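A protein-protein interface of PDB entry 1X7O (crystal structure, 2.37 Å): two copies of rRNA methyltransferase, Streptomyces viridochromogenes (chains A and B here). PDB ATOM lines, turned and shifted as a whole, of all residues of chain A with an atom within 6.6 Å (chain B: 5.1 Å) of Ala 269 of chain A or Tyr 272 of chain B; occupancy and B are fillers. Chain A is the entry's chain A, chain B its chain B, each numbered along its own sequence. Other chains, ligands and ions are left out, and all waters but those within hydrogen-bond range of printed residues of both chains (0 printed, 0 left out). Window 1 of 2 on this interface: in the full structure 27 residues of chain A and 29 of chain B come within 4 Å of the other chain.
The side-chain carboxylate (OE1) of Glu 273 of chain A lies within hydrogen-bond range of the side-chain hydroxyl (OH) of Tyr 272 of chain B, at 2.8 Å.
The side-chain hydroxyl of Tyr 272 of chain A lies within hydrogen-bond range of the side-chain carboxylate of Glu 273 of chain B, 2.7 Å away.
The guanidinium group of Arg 276 of chain A sits close to the guanidinium group of Arg 276 of chain B, 3.3 Å away.
N of Val 218 of chain A sits at hydrogen-bond distance from O of Ser 251 of chain A.
OE2 of Glu 273 of chain B is in salt-bridge range of NH2 of Arg 276 of chain B (3.0 Å).
NH2 of Arg 276 of chain A lies within salt-bridge range of OE2 of Glu 273 of chain A (2.9 Å).
OE2 of Glu 273 of chain A sits at hydrogen-bond distance from NE2 of Gln 277 of chain A (2.8 Å).
Among the printed residues, pairs that only touch across the chains: Val 218 of chain A with Tyr 272 of chain B (3.3 Å), Phe 219 of chain A with Tyr 272 of chain B (3.6 Å), Phe 219 of chain A with Arg 276 of chain B (3.9 Å), Ile 252 of chain A with Leu 150 of chain B (3.8 Å), Pro 253 of chain A with Leu 150 of chain B (3.9 Å), Asn 265 of chain A with Thr 268 of chain B (3.4 Å), Ala 269 of chain A with Tyr 272 of chain B (3.95 Å), Tyr 272 of chain A with Tyr 272 of chain B (3.9 Å), Glu 273 of chain A with Arg 276 of chain B (3.5 Å) and Arg 276 of chain A with Glu 273 of chain B (3.7 Å).
Of the printed residues of chain B, Phe 219 of chain A touches Tyr 272 and Arg 276.
Of the printed residues of chain B, Ile 252 of chain A touches Leu 150 (3.8 Å).
Printed residues of chain B within 4 Å of Pro 253 of chain A: Leu 150.
Of the printed residues of chain B, Arg 276 of chain A touches Glu 273 and Arg 276.
Of the printed residues of chain A, Thr 268 of chain B touches Asn 265.
Tyr 272 of chain B touches just these residues of chain A: Val 218 (3.3 Å), Phe 219 (3.6 Å), Ala 269 (3.95 Å), Tyr 272 (3.9 Å) and Glu 273 (2.8 Å).
Ala 274 of chain B touches none of the printed residues of chain A.
The nearest residue of chain B that does not touch Ala 269 of chain A is Thr 268 of chain B (4.3 Å).
The nearest printed residue of chain B that does not touch Tyr 272 of chain A is Ala 269 of chain B (4.1 Å).
Of the 11 printed residues of chain B, 5 touch a printed residue of chain A.
Along chain B the printed residues that touch a printed residue of chain A span positions 150 to 276.
Of the 22 printed residues of chain A, 9 touch a printed residue of chain B.
Hydrophobic or aromatic side chains of chain A that line the printed part of chain B: Val 218, Phe 219, Ile 252, Ala 269 and Tyr 272.
Along chain A the printed residues that touch a printed residue of chain B span positions 218 to 276.
Among the printed residues, no Asp or Glu carboxylate lies within 4 Å of a Lys or Arg side-chain nitrogen of the other chain.
Ala 269 of chain A touches Tyr 272 of chain B, but with the chains exchanged Tyr 272 of chain A does not touch Ala 269 of chain B (4.1 Å).
Tyr 272 of chain B touches its own counterpart, Tyr 272 of chain A.
Glu 273 of chain A touches Arg 276 of chain B, and with the chains exchanged Arg 276 of chain A touches Glu 273 of chain B.
Arg 276 of chain B touches its own counterpart, Arg 276 of chain A.
10 positions are printed for both chains.
Of the 13 pairs that touch across the chains among the printed residues, 6 have their exchanged pair printed and touching as well.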
ATOM      1  N   LEU A 150     -11.869 -24.300  28.435  1.00  0.00           N
ATOM      2  CA  LEU A 150     -10.494 -24.566  28.846  1.00  0.00           C
ATOM      3  C   LEU A 150     -10.362 -25.071  30.289  1.00  0.00           C
ATOM      4  O   LEU A 150      -9.251 -25.146  30.811  1.00  0.00           O
ATOM      5  CB  LEU A 150      -9.639 -23.312  28.631  1.00  0.00           C
ATOM      6  CG  LEU A 150      -9.410 -22.997  27.147  1.00  0.00           C
ATOM      7  CD1 LEU A 150      -8.874 -21.603  27.004  1.00  0.00           C
ATOM      8  CD2 LEU A 150      -8.450 -23.994  26.513  1.00  0.00           C
ATOM      9  N   ASP A 217       6.370 -12.651  32.902  1.00  0.00           N
ATOM     10  CA  ASP A 217       5.714 -13.275  31.757  1.00  0.00           C
ATOM     11  C   ASP A 217       4.858 -14.431  32.220  1.00  0.00           C
ATOM     12  O   ASP A 217       5.218 -15.142  33.142  1.00  0.00           O
ATOM     13  CB  ASP A 217       6.715 -13.860  30.767  1.00  0.00           C
ATOM     14  CG  ASP A 217       7.567 -12.813  30.064  1.00  0.00           C
ATOM     15  OD1 ASP A 217       7.042 -11.798  29.544  1.00  0.00           O
ATOM     16  OD2 ASP A 217       8.798 -12.970  29.951  1.00  0.00           O
ATOM     17  N   VAL A 218       3.732 -14.618  31.536  1.00  0.00           N
ATOM     18  CA  VAL A 218       2.733 -15.611  31.865  1.00  0.00           C
ATOM     19  C   VAL A 218       3.297 -17.041  31.879  1.00  0.00           C
ATOM     20  O   VAL A 218       2.865 -17.860  32.683  1.00  0.00           O
ATOM     21  CB  VAL A 218       1.518 -15.464  30.891  1.00  0.00           C
ATOM     22  CG1 VAL A 218       1.893 -15.839  29.474  1.00  0.00           C
ATOM     23  CG2 VAL A 218       0.377 -16.265  31.337  1.00  0.00           C
ATOM     24  N   PHE A 219       4.272 -17.327  31.016  1.00  0.00           N
ATOM     25  CA  PHE A 219       4.880 -18.658  30.957  1.00  0.00           C
ATOM     26  C   PHE A 219       5.916 -18.895  32.082  1.00  0.00           C
ATOM     27  O   PHE A 219       6.428 -20.007  32.229  1.00  0.00           O
ATOM     28  CB  PHE A 219       5.492 -18.966  29.558  1.00  0.00           C
ATOM     29  CG  PHE A 219       6.351 -17.859  28.982  1.00  0.00           C
ATOM     30  CD1 PHE A 219       5.850 -17.020  27.985  1.00  0.00           C
ATOM     31  CD2 PHE A 219       7.670 -17.672  29.419  1.00  0.00           C
ATOM     32  CE1 PHE A 219       6.643 -16.002  27.449  1.00  0.00           C
ATOM     33  CE2 PHE A 219       8.469 -16.659  28.896  1.00  0.00           C
ATOM     34  CZ  PHE A 219       7.965 -15.823  27.913  1.00  0.00           C
ATOM     35  N   ASP A 220       6.224 -17.846  32.857  1.00  0.00           N
ATOM     36  CA  ASP A 220       7.084 -17.944  34.052  1.00  0.00           C
ATOM     37  C   ASP A 220       6.278 -17.989  35.353  1.00  0.00           C
ATOM     38  O   ASP A 220       6.839 -17.926  36.435  1.00  0.00           O
ATOM     39  CB  ASP A 220       8.039 -16.750  34.135  1.00  0.00           C
ATOM     40  CG  ASP A 220       9.168 -16.822  33.124  1.00  0.00           C
ATOM     41  OD1 ASP A 220       9.514 -17.930  32.660  1.00  0.00           O
ATOM     42  OD2 ASP A 220       9.791 -15.810  32.744  1.00  0.00           O
ATOM     43  N   SER A 251       2.004 -10.918  32.510  1.00  0.00           N
ATOM     44  CA  SER A 251       1.738 -10.333  31.212  1.00  0.00           C
ATOM     45  C   SER A 251       2.159 -11.210  30.031  1.00  0.00           C
ATOM     46  O   SER A 251       3.123 -11.980  30.111  1.00  0.00           O
ATOM     47  CB  SER A 251       2.430  -8.987  31.117  1.00  0.00           C
ATOM     48  OG  SER A 251       3.824  -9.144  31.201  1.00  0.00           O
ATOM     49  N   ILE A 252       1.428 -11.044  28.932  1.00  0.00           N
ATOM     50  CA  ILE A 252       1.749 -11.673  27.664  1.00  0.00           C
ATOM     51  C   ILE A 252       2.724 -10.755  26.970  1.00  0.00           C
ATOM     52  O   ILE A 252       2.433  -9.585  26.775  1.00  0.00           O
ATOM     53  CB  ILE A 252       0.469 -11.855  26.809  1.00  0.00           C
ATOM     54  CG1 ILE A 252      -0.571 -12.699  27.570  1.00  0.00           C
ATOM     55  CG2 ILE A 252       0.805 -12.479  25.466  1.00  0.00           C
ATOM     56  CD1 ILE A 252      -1.958 -12.729  26.929  1.00  0.00           C
ATOM     57  N   PRO A 253       3.883 -11.272  26.568  1.00  0.00           N
ATOM     58  CA  PRO A 253       4.875 -10.442  25.879  1.00  0.00           C
ATOM     59  C   PRO A 253       4.373  -9.984  24.497  1.00  0.00           C
ATOM     60  O   PRO A 253       3.705 -10.761  23.794  1.00  0.00           O
ATOM     61  CB  PRO A 253       6.066 -11.382  25.727  1.00  0.00           C
ATOM     62  CG  PRO A 253       5.454 -12.724  25.671  1.00  0.00           C
ATOM     63  CD  PRO A 253       4.304 -12.685  26.643  1.00  0.00           C
ATOM     64  N   LEU A 261      -3.956  -6.471  23.254  1.00  0.00           N
ATOM     65  CA  LEU A 261      -4.944  -7.527  23.015  1.00  0.00           C
ATOM     66  C   LEU A 261      -6.297  -7.145  23.583  1.00  0.00           C
ATOM     67  O   LEU A 261      -6.365  -6.552  24.646  1.00  0.00           O
ATOM     68  CB  LEU A 261      -4.510  -8.856  23.646  1.00  0.00           C
ATOM     69  CG  LEU A 261      -3.242  -9.489  23.066  1.00  0.00           C
ATOM     70  CD1 LEU A 261      -2.800 -10.690  23.921  1.00  0.00           C
ATOM     71  CD2 LEU A 261      -3.461  -9.909  21.608  1.00  0.00           C
ATOM     72  N   ALA A 264     -10.875 -10.458  26.072  1.00  0.00           N
ATOM     73  CA  ALA A 264     -11.284 -11.855  25.924  1.00  0.00           C
ATOM     74  C   ALA A 264     -10.201 -12.708  25.268  1.00  0.00           C
ATOM     75  O   ALA A 264     -10.006 -13.857  25.666  1.00  0.00           O
ATOM     76  CB  ALA A 264     -12.589 -11.965  25.119  1.00  0.00           C
ATOM     77  N   ASN A 265      -9.509 -12.132  24.283  1.00  0.00           N
ATOM     78  CA  ASN A 265      -8.403 -12.790  23.596  1.00  0.00           C
ATOM     79  C   ASN A 265      -7.241 -13.033  24.548  1.00  0.00           C
ATOM     80  O   ASN A 265      -6.628 -14.078  24.499  1.00  0.00           O
ATOM     81  CB  ASN A 265      -7.923 -11.956  22.399  1.00  0.00           C
ATOM     82  CG  ASN A 265      -8.890 -12.002  21.215  1.00  0.00           C
ATOM     83  OD1 ASN A 265      -8.824 -11.163  20.311  1.00  0.00           O
ATOM     84  ND2 ASN A 265      -9.782 -12.981  21.207  1.00  0.00           N
ATOM     85  N   ALA A 266      -6.960 -12.061  25.408  1.00  0.00           N
ATOM     86  CA  ALA A 266      -5.912 -12.162  26.398  1.00  0.00           C
ATOM     87  C   ALA A 266      -6.251 -13.259  27.395  1.00  0.00           C
ATOM     88  O   ALA A 266      -5.431 -14.129  27.691  1.00  0.00           O
ATOM     89  CB  ALA A 266      -5.749 -10.818  27.143  1.00  0.00           C
ATOM     90  N   ALA A 267      -7.480 -13.211  27.882  1.00  0.00           N
ATOM     91  CA  ALA A 267      -7.962 -14.164  28.842  1.00  0.00           C
ATOM     92  C   ALA A 267      -7.825 -15.580  28.298  1.00  0.00           C
ATOM     93  O   ALA A 267      -7.386 -16.480  28.997  1.00  0.00           O
ATOM     94  CB  ALA A 267      -9.397 -13.874  29.180  1.00  0.00           C
ATOM     95  N   THR A 268      -8.187 -15.746  27.028  1.00  0.00           N
ATOM     96  CA  THR A 268      -8.149 -17.029  26.392  1.00  0.00           C
ATOM     97  C   THR A 268      -6.720 -17.514  26.340  1.00  0.00           C
ATOM     98  O   THR A 268      -6.458 -18.667  26.675  1.00  0.00           O
ATOM     99  CB  THR A 268      -8.750 -16.951  24.981  1.00  0.00           C
ATOM    100  OG1 THR A 268     -10.138 -16.599  25.071  1.00  0.00           O
ATOM    101  CG2 THR A 268      -8.727 -18.327  24.296  1.00  0.00           C
ATOM    102  N   ALA A 269      -5.787 -16.640  25.965  1.00  0.00           N
ATOM    103  CA  ALA A 269      -4.401 -17.054  25.866  1.00  0.00           C
ATOM    104  C   ALA A 269      -3.838 -17.433  27.220  1.00  0.00           C
ATOM    105  O   ALA A 269      -3.094 -18.400  27.313  1.00  0.00           O
ATOM    106  CB  ALA A 269      -3.561 -15.991  25.225  1.00  0.00           C
ATOM    107  N   ILE A 270      -4.200 -16.698  28.266  1.00  0.00           N
ATOM    108  CA  ILE A 270      -3.647 -16.933  29.601  1.00  0.00           C
ATOM    109  C   ILE A 270      -4.285 -18.170  30.239  1.00  0.00           C
ATOM    110  O   ILE A 270      -3.652 -18.896  30.951  1.00  0.00           O
ATOM    111  CB  ILE A 270      -3.807 -15.685  30.504  1.00  0.00           C
ATOM    112  CG1 ILE A 270      -2.927 -14.528  29.999  1.00  0.00           C
ATOM    113  CG2 ILE A 270      -3.475 -16.004  31.947  1.00  0.00           C
ATOM    114  CD1 ILE A 270      -3.221 -13.172  30.684  1.00  0.00           C
ATOM    115  N   LEU A 271      -5.541 -18.415  29.953  1.00  0.00           N
ATOM    116  CA  LEU A 271      -6.183 -19.648  30.374  1.00  0.00           C
ATOM    117  C   LEU A 271      -5.557 -20.838  29.656  1.00  0.00           C
ATOM    118  O   LEU A 271      -5.310 -21.864  30.270  1.00  0.00           O
ATOM    119  CB  LEU A 271      -7.671 -19.601  30.050  1.00  0.00           C
ATOM    120  CG  LEU A 271      -8.752 -19.426  31.100  1.00  0.00           C
ATOM    121  CD1 LEU A 271      -8.286 -19.128  32.533  1.00  0.00           C
ATOM    122  CD2 LEU A 271      -9.780 -18.395  30.600  1.00  0.00           C
ATOM    123  N   TYR A 272      -5.304 -20.718  28.356  1.00  0.00           N
ATOM    124  CA  TYR A 272      -4.641 -21.786  27.608  1.00  0.00           C
ATOM    125  C   TYR A 272      -3.271 -22.097  28.226  1.00  0.00           C
ATOM    126  O   TYR A 272      -2.871 -23.252  28.295  1.00  0.00           O
ATOM    127  CB  TYR A 272      -4.478 -21.440  26.112  1.00  0.00           C
ATOM    128  CG  TYR A 272      -3.310 -22.159  25.500  1.00  0.00           C
ATOM    129  CD1 TYR A 272      -3.439 -23.468  25.051  1.00  0.00           C
ATOM    130  CD2 TYR A 272      -2.058 -21.581  25.465  1.00  0.00           C
ATOM    131  CE1 TYR A 272      -2.342 -24.178  24.533  1.00  0.00           C
ATOM    132  CE2 TYR A 272      -0.962 -22.273  24.953  1.00  0.00           C
ATOM    133  CZ  TYR A 272      -1.109 -23.575  24.492  1.00  0.00           C
ATOM    134  OH  TYR A 272      -0.019 -24.269  23.981  1.00  0.00           O
ATOM    135  N   GLU A 273      -2.562 -21.076  28.697  1.00  0.00           N
ATOM    136  CA  GLU A 273      -1.225 -21.296  29.259  1.00  0.00           C
ATOM    137  C   GLU A 273      -1.311 -22.063  30.578  1.00  0.00           C
ATOM    138  O   GLU A 273      -0.404 -22.860  30.891  1.00  0.00           O
ATOM    139  CB  GLU A 273      -0.497 -19.972  29.456  1.00  0.00           C
ATOM    140  CG  GLU A 273       0.760 -20.017  30.314  1.00  0.00           C
ATOM    141  CD  GLU A 273       1.897 -20.874  29.741  1.00  0.00           C
ATOM    142  OE1 GLU A 273       2.009 -21.076  28.490  1.00  0.00           O
ATOM    143  OE2 GLU A 273       2.724 -21.328  30.568  1.00  0.00           O
ATOM    144  N   ALA A 274      -2.376 -21.800  31.352  1.00  0.00           N
ATOM    145  CA  ALA A 274      -2.640 -22.545  32.583  1.00  0.00           C
ATOM    146  C   ALA A 274      -2.916 -24.021  32.258  1.00  0.00           C
ATOM    147  O   ALA A 274      -2.261 -24.905  32.809  1.00  0.00           O
ATOM    148  CB  ALA A 274      -3.784 -21.934  33.363  1.00  0.00           C
ATOM    149  N   ARG A 276      -1.905 -25.600  29.608  1.00  0.00           N
ATOM    150  CA  ARG A 276      -0.674 -26.197  29.097  1.00  0.00           C
ATOM    151  C   ARG A 276       0.242 -26.681  30.230  1.00  0.00           C
ATOM    152  O   ARG A 276       0.754 -27.791  30.176  1.00  0.00           O
ATOM    153  CB  ARG A 276       0.075 -25.207  28.204  1.00  0.00           C
ATOM    154  CG  ARG A 276       1.307 -25.782  27.513  1.00  0.00           C
ATOM    155  CD  ARG A 276       2.295 -24.719  27.016  1.00  0.00           C
ATOM    156  NE  ARG A 276       2.911 -23.963  28.109  1.00  0.00           N
ATOM    157  CZ  ARG A 276       4.055 -24.288  28.726  1.00  0.00           C
ATOM    158  NH1 ARG A 276       4.754 -25.380  28.384  1.00  0.00           N
ATOM    159  NH2 ARG A 276       4.516 -23.503  29.700  1.00  0.00           N
ATOM    160  N   GLN A 277       0.439 -25.845  31.250  1.00  0.00           N
ATOM    161  CA  GLN A 277       1.281 -26.209  32.399  1.00  0.00           C
ATOM    162  C   GLN A 277       0.634 -27.288  33.264  1.00  0.00           C
ATOM    163  O   GLN A 277       1.335 -28.025  33.937  1.00  0.00           O
ATOM    164  CB  GLN A 277       1.567 -25.003  33.308  1.00  0.00           C
ATOM    165  CG  GLN A 277       2.477 -23.897  32.747  1.00  0.00           C
ATOM    166  CD  GLN A 277       2.681 -22.822  33.784  1.00  0.00           C
ATOM    167  OE1 GLN A 277       2.593 -23.115  34.971  1.00  0.00           O
ATOM    168  NE2 GLN A 277       2.858 -21.556  33.351  1.00  0.00           N
ATOM    169  N   LEU B 150       1.137 -10.022  18.717  1.00  0.00           N
ATOM    170  CA  LEU B 150       1.924 -11.216  18.981  1.00  0.00           C
ATOM    171  C   LEU B 150       2.977 -11.569  17.883  1.00  0.00           C
ATOM    172  O   LEU B 150       3.314 -12.745  17.673  1.00  0.00           O
ATOM    173  CB  LEU B 150       0.970 -12.380  19.198  1.00  0.00           C
ATOM    174  CG  LEU B 150       0.051 -12.221  20.403  1.00  0.00           C
ATOM    175  CD1 LEU B 150      -1.053 -13.196  20.338  1.00  0.00           C
ATOM    176  CD2 LEU B 150       0.806 -12.415  21.682  1.00  0.00           C
ATOM    177  N   ALA B 267      -7.381 -18.385  17.664  1.00  0.00           N
ATOM    178  CA  ALA B 267      -6.237 -17.906  16.884  1.00  0.00           C
ATOM    179  C   ALA B 267      -5.229 -17.185  17.770  1.00  0.00           C
ATOM    180  O   ALA B 267      -4.021 -17.355  17.595  1.00  0.00           O
ATOM    181  CB  ALA B 267      -6.697 -16.997  15.766  1.00  0.00           C
ATOM    182  N   THR B 268      -5.742 -16.399  18.721  1.00  0.00           N
ATOM    183  CA  THR B 268      -4.916 -15.713  19.712  1.00  0.00           C
ATOM    184  C   THR B 268      -4.130 -16.681  20.581  1.00  0.00           C
ATOM    185  O   THR B 268      -2.954 -16.485  20.801  1.00  0.00           O
ATOM    186  CB  THR B 268      -5.764 -14.823  20.627  1.00  0.00           C
ATOM    187  OG1 THR B 268      -6.373 -13.770  19.868  1.00  0.00           O
ATOM    188  CG2 THR B 268      -4.875 -14.102  21.637  1.00  0.00           C
ATOM    189  N   ALA B 269      -4.771 -17.736  21.052  1.00  0.00           N
ATOM    190  CA  ALA B 269      -4.104 -18.699  21.909  1.00  0.00           C
ATOM    191  C   ALA B 269      -2.952 -19.394  21.167  1.00  0.00           C
ATOM    192  O   ALA B 269      -1.877 -19.630  21.741  1.00  0.00           O
ATOM    193  CB  ALA B 269      -5.111 -19.712  22.431  1.00  0.00           C
ATOM    194  N   ILE B 270      -3.153 -19.687  19.883  1.00  0.00           N
ATOM    195  CA  ILE B 270      -2.171 -20.446  19.094  1.00  0.00           C
ATOM    196  C   ILE B 270      -0.983 -19.565  18.720  1.00  0.00           C
ATOM    197  O   ILE B 270       0.149 -19.992  18.730  1.00  0.00           O
ATOM    198  CB  ILE B 270      -2.837 -21.012  17.808  1.00  0.00           C
ATOM    199  CG1 ILE B 270      -3.920 -22.035  18.172  1.00  0.00           C
ATOM    200  CG2 ILE B 270      -1.794 -21.609  16.877  1.00  0.00           C
ATOM    201  CD1 ILE B 270      -4.755 -22.512  16.975  1.00  0.00           C
ATOM    202  N   LEU B 271      -1.272 -18.336  18.338  1.00  0.00           N
ATOM    203  CA  LEU B 271      -0.242 -17.326  18.160  1.00  0.00           C
ATOM    204  C   LEU B 271       0.568 -17.102  19.446  1.00  0.00           C
ATOM    205  O   LEU B 271       1.779 -16.897  19.367  1.00  0.00           O
ATOM    206  CB  LEU B 271      -0.872 -15.999  17.769  1.00  0.00           C
ATOM    207  CG  LEU B 271      -0.934 -15.542  16.317  1.00  0.00           C
ATOM    208  CD1 LEU B 271      -0.323 -16.506  15.338  1.00  0.00           C
ATOM    209  CD2 LEU B 271      -2.343 -15.164  15.910  1.00  0.00           C
ATOM    210  N   TYR B 272      -0.094 -17.101  20.613  1.00  0.00           N
ATOM    211  CA  TYR B 272       0.611 -16.920  21.871  1.00  0.00           C
ATOM    212  C   TYR B 272       1.563 -18.106  22.072  1.00  0.00           C
ATOM    213  O   TYR B 272       2.667 -17.933  22.558  1.00  0.00           O
ATOM    214  CB  TYR B 272      -0.342 -16.814  23.085  1.00  0.00           C
ATOM    215  CG  TYR B 272       0.379 -17.245  24.335  1.00  0.00           C
ATOM    216  CD1 TYR B 272       1.371 -16.440  24.898  1.00  0.00           C
ATOM    217  CD2 TYR B 272       0.157 -18.479  24.886  1.00  0.00           C
ATOM    218  CE1 TYR B 272       2.088 -16.849  25.997  1.00  0.00           C
ATOM    219  CE2 TYR B 272       0.868 -18.896  26.002  1.00  0.00           C
ATOM    220  CZ  TYR B 272       1.834 -18.076  26.544  1.00  0.00           C
ATOM    221  OH  TYR B 272       2.536 -18.482  27.636  1.00  0.00           O
ATOM    222  N   GLU B 273       1.124 -19.307  21.714  1.00  0.00           N
ATOM    223  CA  GLU B 273       1.947 -20.518  21.847  1.00  0.00           C
ATOM    224  C   GLU B 273       3.164 -20.443  20.941  1.00  0.00           C
ATOM    225  O   GLU B 273       4.252 -20.881  21.300  1.00  0.00           O
ATOM    226  CB  GLU B 273       1.112 -21.763  21.506  1.00  0.00           C
ATOM    227  CG  GLU B 273       1.874 -23.077  21.372  1.00  0.00           C
ATOM    228  CD  GLU B 273       2.631 -23.453  22.631  1.00  0.00           C
ATOM    229  OE1 GLU B 273       2.292 -22.936  23.719  1.00  0.00           O
ATOM    230  OE2 GLU B 273       3.576 -24.252  22.536  1.00  0.00           O
ATOM    231  N   ALA B 274       2.978 -19.880  19.757  1.00  0.00           N
ATOM    232  CA  ALA B 274       4.087 -19.713  18.816  1.00  0.00           C
ATOM    233  C   ALA B 274       5.123 -18.728  19.354  1.00  0.00           C
ATOM    234  O   ALA B 274       6.315 -19.024  19.330  1.00  0.00           O
ATOM    235  CB  ALA B 274       3.583 -19.264  17.476  1.00  0.00           C
ATOM    236  N   VAL B 275       4.658 -17.569  19.838  1.00  0.00           N
ATOM    237  CA  VAL B 275       5.512 -16.609  20.549  1.00  0.00           C
ATOM    238  C   VAL B 275       6.243 -17.294  21.719  1.00  0.00           C
ATOM    239  O   VAL B 275       7.428 -17.133  21.888  1.00  0.00           O
ATOM    240  CB  VAL B 275       4.711 -15.424  21.139  1.00  0.00           C
ATOM    241  CG1 VAL B 275       5.633 -14.500  21.892  1.00  0.00           C
ATOM    242  CG2 VAL B 275       3.988 -14.616  20.065  1.00  0.00           C
ATOM    243  N   ARG B 276       5.529 -18.075  22.518  1.00  0.00           N
ATOM    244  CA  ARG B 276       6.149 -18.695  23.685  1.00  0.00           C
ATOM    245  C   ARG B 276       7.338 -19.583  23.291  1.00  0.00           C
ATOM    246  O   ARG B 276       8.395 -19.501  23.894  1.00  0.00           O
ATOM    247  CB  ARG B 276       5.100 -19.477  24.479  1.00  0.00           C
ATOM    248  CG  ARG B 276       5.627 -20.186  25.700  1.00  0.00           C
ATOM    249  CD  ARG B 276       4.689 -21.244  26.266  1.00  0.00           C
ATOM    250  NE  ARG B 276       4.681 -22.463  25.477  1.00  0.00           N
ATOM    251  CZ  ARG B 276       5.576 -23.459  25.596  1.00  0.00           C
ATOM    252  NH1 ARG B 276       6.585 -23.398  26.465  1.00  0.00           N
ATOM    253  NH2 ARG B 276       5.455 -24.538  24.835  1.00  0.00           N
